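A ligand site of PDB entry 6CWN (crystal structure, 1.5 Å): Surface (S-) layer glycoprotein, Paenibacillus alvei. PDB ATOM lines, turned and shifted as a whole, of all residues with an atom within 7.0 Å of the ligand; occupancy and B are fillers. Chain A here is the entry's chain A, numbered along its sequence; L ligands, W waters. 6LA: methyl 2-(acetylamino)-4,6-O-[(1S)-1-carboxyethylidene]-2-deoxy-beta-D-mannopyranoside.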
ATOM      1  N   PHE A  15      -0.176  16.951   5.555  1.00  0.00           N
ATOM      2  CA  PHE A  15       0.363  15.610   5.467  1.00  0.00           C
ATOM      3  C   PHE A  15       1.318  15.445   4.298  1.00  0.00           C
ATOM      4  O   PHE A  15       2.426  14.941   4.490  1.00  0.00           O
ATOM      5  CB  PHE A  15      -0.762  14.595   5.444  1.00  0.00           C
ATOM      6  CG  PHE A  15      -0.294  13.195   5.213  1.00  0.00           C
ATOM      7  CD1 PHE A  15      -0.043  12.769   3.920  1.00  0.00           C
ATOM      8  CD2 PHE A  15      -0.058  12.324   6.282  1.00  0.00           C
ATOM      9  CE1 PHE A  15       0.397  11.462   3.677  1.00  0.00           C
ATOM     10  CE2 PHE A  15       0.412  11.008   6.033  1.00  0.00           C
ATOM     11  CZ  PHE A  15       0.638  10.601   4.713  1.00  0.00           C
ATOM     12  N   GLY A  22       9.801  13.792   5.131  1.00  0.00           N
ATOM     13  CA  GLY A  22      10.185  12.568   5.773  1.00  0.00           C
ATOM     14  C   GLY A  22       9.618  12.301   7.170  1.00  0.00           C
ATOM     15  O   GLY A  22       9.948  11.296   7.783  1.00  0.00           O
ATOM     16  N   VAL A  23       8.708  13.143   7.631  1.00  0.00           N
ATOM     17  CA  VAL A  23       8.127  13.013   8.972  1.00  0.00           C
ATOM     18  C   VAL A  23       7.018  12.001   8.954  1.00  0.00           C
ATOM     19  O   VAL A  23       6.884  11.208   9.896  1.00  0.00           O
ATOM     20  CB  VAL A  23       7.641  14.348   9.502  1.00  0.00           C
ATOM     21  CG1 VAL A  23       6.915  14.206  10.837  1.00  0.00           C
ATOM     22  CG2 VAL A  23       8.796  15.333   9.681  1.00  0.00           C
ATOM     23  N   PHE A  24       6.178  12.069   7.930  1.00  0.00           N
ATOM     24  CA  PHE A  24       5.244  11.043   7.640  1.00  0.00           C
ATOM     25  C   PHE A  24       5.622  10.231   6.423  1.00  0.00           C
ATOM     26  O   PHE A  24       6.339  10.725   5.568  1.00  0.00           O
ATOM     27  CB  PHE A  24       3.781  11.620   7.446  1.00  0.00           C
ATOM     28  CG  PHE A  24       3.084  11.985   8.738  1.00  0.00           C
ATOM     29  CD1 PHE A  24       3.375  13.175   9.424  1.00  0.00           C
ATOM     30  CD2 PHE A  24       2.164  11.116   9.273  1.00  0.00           C
ATOM     31  CE1 PHE A  24       2.715  13.482  10.616  1.00  0.00           C
ATOM     32  CE2 PHE A  24       1.514  11.450  10.475  1.00  0.00           C
ATOM     33  CZ  PHE A  24       1.817  12.621  11.107  1.00  0.00           C
ATOM     34  N   SER A  25       5.047   9.043   6.321  1.00  0.00           N
ATOM     35  CA  SER A  25       5.221   8.153   5.156  1.00  0.00           C
ATOM     36  C   SER A  25       3.939   7.516   4.656  1.00  0.00           C
ATOM     37  O   SER A  25       3.930   6.975   3.548  1.00  0.00           O
ATOM     38  CB  SER A  25       6.272   7.103   5.434  1.00  0.00           C
ATOM     39  OG  SER A  25       5.705   6.169   6.299  1.00  0.00           O
ATOM     40  N   GLY A  26       2.821   7.665   5.402  1.00  0.00           N
ATOM     41  CA  GLY A  26       1.646   6.902   5.153  1.00  0.00           C
ATOM     42  C   GLY A  26       1.829   5.395   5.336  1.00  0.00           C
ATOM     43  O   GLY A  26       2.748   4.956   6.059  1.00  0.00           O
ATOM     44  N   TYR A  27       0.895   4.641   4.780  1.00  0.00           N
ATOM     45  CA  TYR A  27       0.814   3.179   4.887  1.00  0.00           C
ATOM     46  C   TYR A  27       1.372   2.531   3.652  1.00  0.00           C
ATOM     47  O   TYR A  27       1.274   3.094   2.521  1.00  0.00           O
ATOM     48  CB  TYR A  27      -0.592   2.693   5.180  1.00  0.00           C
ATOM     49  CG  TYR A  27      -1.156   3.226   6.493  1.00  0.00           C
ATOM     50  CD1 TYR A  27      -1.813   4.464   6.549  1.00  0.00           C
ATOM     51  CD2 TYR A  27      -1.048   2.476   7.669  1.00  0.00           C
ATOM     52  CE1 TYR A  27      -2.285   4.921   7.761  1.00  0.00           C
ATOM     53  CE2 TYR A  27      -1.534   2.910   8.864  1.00  0.00           C
ATOM     54  CZ  TYR A  27      -2.143   4.124   8.907  1.00  0.00           C
ATOM     55  OH  TYR A  27      -2.584   4.601  10.126  1.00  0.00           O
ATOM     56  N   PRO A  28       1.964   1.330   3.813  1.00  0.00           N
ATOM     57  CA  PRO A  28       2.466   0.645   2.650  1.00  0.00           C
ATOM     58  C   PRO A  28       1.391   0.314   1.633  1.00  0.00           C
ATOM     59  O   PRO A  28       0.293  -0.097   1.969  1.00  0.00           O
ATOM     60  CB  PRO A  28       3.038  -0.642   3.210  1.00  0.00           C
ATOM     61  CG  PRO A  28       3.189  -0.440   4.662  1.00  0.00           C
ATOM     62  CD  PRO A  28       2.246   0.623   5.071  1.00  0.00           C
ATOM     63  N   GLY A  29       1.705   0.595   0.398  1.00  0.00           N
ATOM     64  CA  GLY A  29       0.882   0.147  -0.737  1.00  0.00           C
ATOM     65  C   GLY A  29      -0.392   0.941  -0.949  1.00  0.00           C
ATOM     66  O   GLY A  29      -1.245   0.483  -1.700  1.00  0.00           O
ATOM     67  N   ALA A  33      -3.964   8.310   3.562  1.00  0.00           N
ATOM     68  CA  ALA A  33      -3.370   8.697   4.821  1.00  0.00           C
ATOM     69  C   ALA A  33      -4.168   8.373   6.046  1.00  0.00           C
ATOM     70  O   ALA A  33      -3.615   8.461   7.178  1.00  0.00           O
ATOM     71  CB  ALA A  33      -3.073  10.202   4.849  1.00  0.00           C
ATOM     72  N   MET A  39      -4.948   7.853  15.909  1.00  0.00           N
ATOM     73  CA  MET A  39      -3.512   7.482  15.828  1.00  0.00           C
ATOM     74  C   MET A  39      -3.155   6.448  16.885  1.00  0.00           C
ATOM     75  O   MET A  39      -3.672   6.491  18.011  1.00  0.00           O
ATOM     76  CB  MET A  39      -2.580   8.701  15.948  1.00  0.00           C
ATOM     77  CG  MET A  39      -1.137   8.366  15.595  1.00  0.00           C
ATOM     78  SD  MET A  39       0.054   9.749  15.457  1.00  0.00           S
ATOM     79  CE  MET A  39      -0.137  10.211  13.746  1.00  0.00           C
ATOM     80  N   THR A  40      -2.263   5.509  16.556  1.00  0.00           N
ATOM     81  CA  THR A  40      -1.754   4.602  17.540  1.00  0.00           C
ATOM     82  C   THR A  40      -0.491   5.085  18.242  1.00  0.00           C
ATOM     83  O   THR A  40       0.196   6.009  17.795  1.00  0.00           O
ATOM     84  CB  THR A  40      -1.462   3.251  16.965  1.00  0.00           C
ATOM     85  OG1 THR A  40      -0.345   3.372  16.090  1.00  0.00           O
ATOM     86  CG2 THR A  40      -2.628   2.658  16.254  1.00  0.00           C
ATOM     87  N   ALA A  42       2.281   3.408  18.490  1.00  0.00           N
ATOM     88  CA  ALA A  42       3.383   3.122  17.579  1.00  0.00           C
ATOM     89  C   ALA A  42       3.551   4.240  16.569  1.00  0.00           C
ATOM     90  O   ALA A  42       4.693   4.686  16.279  1.00  0.00           O
ATOM     91  CB  ALA A  42       3.151   1.833  16.859  1.00  0.00           C
ATOM     92  N   GLU A  43       2.482   4.698  15.984  1.00  0.00           N
ATOM     93  CA  GLU A  43       2.555   5.762  14.970  1.00  0.00           C
ATOM     94  C   GLU A  43       3.040   7.064  15.578  1.00  0.00           C
ATOM     95  O   GLU A  43       3.875   7.803  14.993  1.00  0.00           O
ATOM     96  CB  GLU A  43       1.177   5.959  14.330  1.00  0.00           C
ATOM     97  CG  GLU A  43       0.752   4.802  13.432  1.00  0.00           C
ATOM     98  CD  GLU A  43      -0.687   4.779  12.943  1.00  0.00           C
ATOM     99  OE1 GLU A  43      -1.472   5.648  13.391  1.00  0.00           O
ATOM    100  OE2 GLU A  43      -0.960   3.879  12.115  1.00  0.00           O
ATOM    101  N   PHE A  44       2.588   7.375  16.801  1.00  0.00           N
ATOM    102  CA  PHE A  44       3.021   8.601  17.459  1.00  0.00           C
ATOM    103  C   PHE A  44       4.518   8.499  17.763  1.00  0.00           C
ATOM    104  O   PHE A  44       5.243   9.486  17.579  1.00  0.00           O
ATOM    105  CB  PHE A  44       2.191   8.798  18.729  1.00  0.00           C
ATOM    106  CG  PHE A  44       2.469  10.075  19.469  1.00  0.00           C
ATOM    107  CD1 PHE A  44       2.361  11.257  18.886  1.00  0.00           C
ATOM    108  CD2 PHE A  44       2.657  10.062  20.823  1.00  0.00           C
ATOM    109  CE1 PHE A  44       2.552  12.465  19.558  1.00  0.00           C
ATOM    110  CE2 PHE A  44       2.794  11.228  21.514  1.00  0.00           C
ATOM    111  CZ  PHE A  44       2.728  12.403  20.905  1.00  0.00           C
ATOM    112  N   LYS A  46       6.810   6.970  16.057  1.00  0.00           N
ATOM    113  CA  LYS A  46       7.506   7.244  14.796  1.00  0.00           C
ATOM    114  C   LYS A  46       7.556   8.764  14.524  1.00  0.00           C
ATOM    115  O   LYS A  46       8.628   9.344  14.180  1.00  0.00           O
ATOM    116  CB  LYS A  46       6.870   6.469  13.663  1.00  0.00           C
ATOM    117  CG  LYS A  46       7.643   6.380  12.367  1.00  0.00           C
ATOM    118  CD  LYS A  46       7.812   7.606  11.627  1.00  0.00           C
ATOM    119  CE  LYS A  46       6.608   8.067  10.914  1.00  0.00           C
ATOM    120  NZ  LYS A  46       6.488   7.590   9.448  1.00  0.00           N
ATOM    121  N   VAL A  47       6.411   9.439  14.618  1.00  0.00           N
ATOM    122  CA  VAL A  47       6.341  10.841  14.296  1.00  0.00           C
ATOM    123  C   VAL A  47       7.253  11.618  15.261  1.00  0.00           C
ATOM    124  O   VAL A  47       7.981  12.527  14.847  1.00  0.00           O
ATOM    125  CB  VAL A  47       4.871  11.328  14.369  1.00  0.00           C
ATOM    126  CG1 VAL A  47       4.808  12.863  14.239  1.00  0.00           C
ATOM    127  CG2 VAL A  47       4.083  10.668  13.227  1.00  0.00           C
ATOM    128  N   LYS A  50      10.924  11.316  14.122  1.00  0.00           N
ATOM    129  CA  LYS A  50      11.232  12.101  12.924  1.00  0.00           C
ATOM    130  C   LYS A  50      11.192  13.604  13.213  1.00  0.00           C
ATOM    131  O   LYS A  50      12.102  14.356  12.770  1.00  0.00           O
ATOM    132  CB  LYS A  50      10.209  11.756  11.860  1.00  0.00           C
ATOM    133  CG  LYS A  50      10.276  10.342  11.317  1.00  0.00           C
ATOM    134  CD  LYS A  50      11.566  10.009  10.633  1.00  0.00           C
ATOM    135  CE  LYS A  50      11.430   8.636  10.056  1.00  0.00           C
ATOM    136  NZ  LYS A  50      12.669   8.174   9.378  1.00  0.00           N
ATOM    137  N   TRP A  73       7.608  -3.008  12.720  1.00  0.00           N
ATOM    138  CA  TRP A  73       8.205  -1.832  12.155  1.00  0.00           C
ATOM    139  C   TRP A  73       8.431  -0.744  13.170  1.00  0.00           C
ATOM    140  O   TRP A  73       9.274   0.092  13.006  1.00  0.00           O
ATOM    141  CB  TRP A  73       7.320  -1.248  10.981  1.00  0.00           C
ATOM    142  CG  TRP A  73       6.015  -0.728  11.399  1.00  0.00           C
ATOM    143  CD1 TRP A  73       4.832  -1.411  11.447  1.00  0.00           C
ATOM    144  CD2 TRP A  73       5.758   0.570  11.928  1.00  0.00           C
ATOM    145  NE1 TRP A  73       3.846  -0.611  11.949  1.00  0.00           N
ATOM    146  CE2 TRP A  73       4.390   0.596  12.288  1.00  0.00           C
ATOM    147  CE3 TRP A  73       6.550   1.697  12.171  1.00  0.00           C
ATOM    148  CZ2 TRP A  73       3.797   1.725  12.851  1.00  0.00           C
ATOM    149  CZ3 TRP A  73       5.919   2.801  12.715  1.00  0.00           C
ATOM    150  CH2 TRP A  73       4.595   2.780  13.102  1.00  0.00           C
ATOM    151  N   PHE A  77      11.464   2.826  16.765  1.00  0.00           N
ATOM    152  CA  PHE A  77      10.925   4.116  17.161  1.00  0.00           C
ATOM    153  C   PHE A  77      10.459   4.132  18.633  1.00  0.00           C
ATOM    154  O   PHE A  77      10.749   5.080  19.340  1.00  0.00           O
ATOM    155  CB  PHE A  77       9.797   4.547  16.230  1.00  0.00           C
ATOM    156  CG  PHE A  77      10.219   4.570  14.752  1.00  0.00           C
ATOM    157  CD1 PHE A  77      10.989   5.603  14.258  1.00  0.00           C
ATOM    158  CD2 PHE A  77       9.913   3.537  13.922  1.00  0.00           C
ATOM    159  CE1 PHE A  77      11.385   5.662  12.963  1.00  0.00           C
ATOM    160  CE2 PHE A  77      10.340   3.576  12.586  1.00  0.00           C
ATOM    161  CZ  PHE A  77      11.074   4.634  12.124  1.00  0.00           C
ATOM    162  N   ARG A 157      -5.391  10.868  13.589  1.00  0.00           N
ATOM    163  CA  ARG A 157      -4.233  11.118  12.749  1.00  0.00           C
ATOM    164  C   ARG A 157      -4.218  12.537  12.192  1.00  0.00           C
ATOM    165  O   ARG A 157      -3.154  13.176  12.170  1.00  0.00           O
ATOM    166  CB  ARG A 157      -4.127  10.066  11.669  1.00  0.00           C
ATOM    167  CG  ARG A 157      -3.739   8.661  12.150  1.00  0.00           C
ATOM    168  CD  ARG A 157      -3.799   7.570  11.098  1.00  0.00           C
ATOM    169  NE  ARG A 157      -3.017   7.912   9.941  1.00  0.00           N
ATOM    170  CZ  ARG A 157      -1.682   7.771   9.848  1.00  0.00           C
ATOM    171  NH1 ARG A 157      -0.945   7.347  10.910  1.00  0.00           N
ATOM    172  NH2 ARG A 157      -1.093   8.111   8.703  1.00  0.00           N
HETATM  173  C8  6LA L   1       5.384   3.239   4.760  1.00  0.00           C
HETATM  174  C7  6LA L   1       5.619   2.767   6.193  1.00  0.00           C
HETATM  175  O7  6LA L   1       6.555   2.035   6.451  1.00  0.00           O
HETATM  176  N2  6LA L   1       4.700   3.138   7.055  1.00  0.00           N
HETATM  177  C2  6LA L   1       4.828   2.750   8.427  1.00  0.00           C
HETATM  178  C3  6LA L   1       5.052   3.948   9.351  1.00  0.00           C
HETATM  179  O3  6LA L   1       6.198   4.720   9.022  1.00  0.00           O
HETATM  180  C4  6LA L   1       3.801   4.839   9.291  1.00  0.00           C
HETATM  181  O4  6LA L   1       3.892   5.888  10.268  1.00  0.00           O
HETATM  182  CAB 6LA L   1       2.773   6.802  10.227  1.00  0.00           C
HETATM  183  CAK 6LA L   1       2.961   7.788  11.381  1.00  0.00           C
HETATM  184  CAL 6LA L   1       2.798   7.571   8.855  1.00  0.00           C
HETATM  185  OAN 6LA L   1       3.932   7.999   8.497  1.00  0.00           O
HETATM  186  OAM 6LA L   1       1.717   7.808   8.307  1.00  0.00           O
HETATM  187  O6  6LA L   1       1.584   6.080  10.393  1.00  0.00           O
HETATM  188  C6  6LA L   1       1.338   4.956   9.569  1.00  0.00           C
HETATM  189  C5  6LA L   1       2.624   4.047   9.614  1.00  0.00           C
HETATM  190  O5  6LA L   1       2.438   2.962   8.743  1.00  0.00           O
HETATM  191  C1  6LA L   1       3.547   2.075   8.878  1.00  0.00           C
HETATM  192  O1  6LA L   1       3.331   0.948   8.125  1.00  0.00           O
HETATM  193  CAU 6LA L   1       2.286   0.102   8.562  1.00  0.00           C
HETATM  194  O   HOH W   1      -0.609  -0.389  10.434  1.00  0.00           O
HETATM  195  O   HOH W   2       8.433   2.989   8.958  1.00  0.00           O
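Merely in contact with the ligand: Pro 28 (3.3 Å), Glu 43 (3.4 Å), Phe 24 (3.4 Å), Tyr 27 (3.6 Å), Val 47 (3.6 Å) and Trp 73 (3.7 Å). Within 4 Å of the ligand: Phe 24, Ser 25, Gly 26, Tyr 27, Pro 28, Glu 43, Lys 46, Val 47, Trp 73 and Arg 157. The nearest printed residue that does not touch the ligand is Phe 15 (4.1 Å).
An oxygen (OAN) of the ligand sits at hydrogen-bond distance from the backbone NH (N) of Ser 25 (2.7 Å). NZ of Lys 46 is in salt-bridge range of OAN of the ligand (2.8 Å). O of Gly 26 is in hydrogen-bond range of N2 of the ligand (2.8 Å). The backbone NH (N) of Gly 26 lies within hydrogen-bond range of an oxygen (OAM) of the ligand, 3.1 Å away. OG of Ser 25 lies within hydrogen-bond range of O3 of the ligand, at 3.1 Å. OAM of the ligand lies within salt-bridge range of NH2 of Arg 157, 2.9 Å away.
OG1 of Thr 40 lies within hydrogen-bond range of N of Glu 43, at 3.1 Å. NH1 of Arg 157 sits at hydrogen-bond distance from OH of Tyr 27, at 3.3 Å. OE2 of Glu 43 sits at hydrogen-bond distance from OH of Tyr 27 (2.7 Å). The guanidinium group (NH1) of Arg 157 is in salt-bridge range of the side-chain carboxylate (OE1) of Glu 43 (3.1 Å). The guanidinium group of Arg 157 lies within hydrogen-bond range of the backbone carbonyl oxygen of Ala 33, at 2.9 Å.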
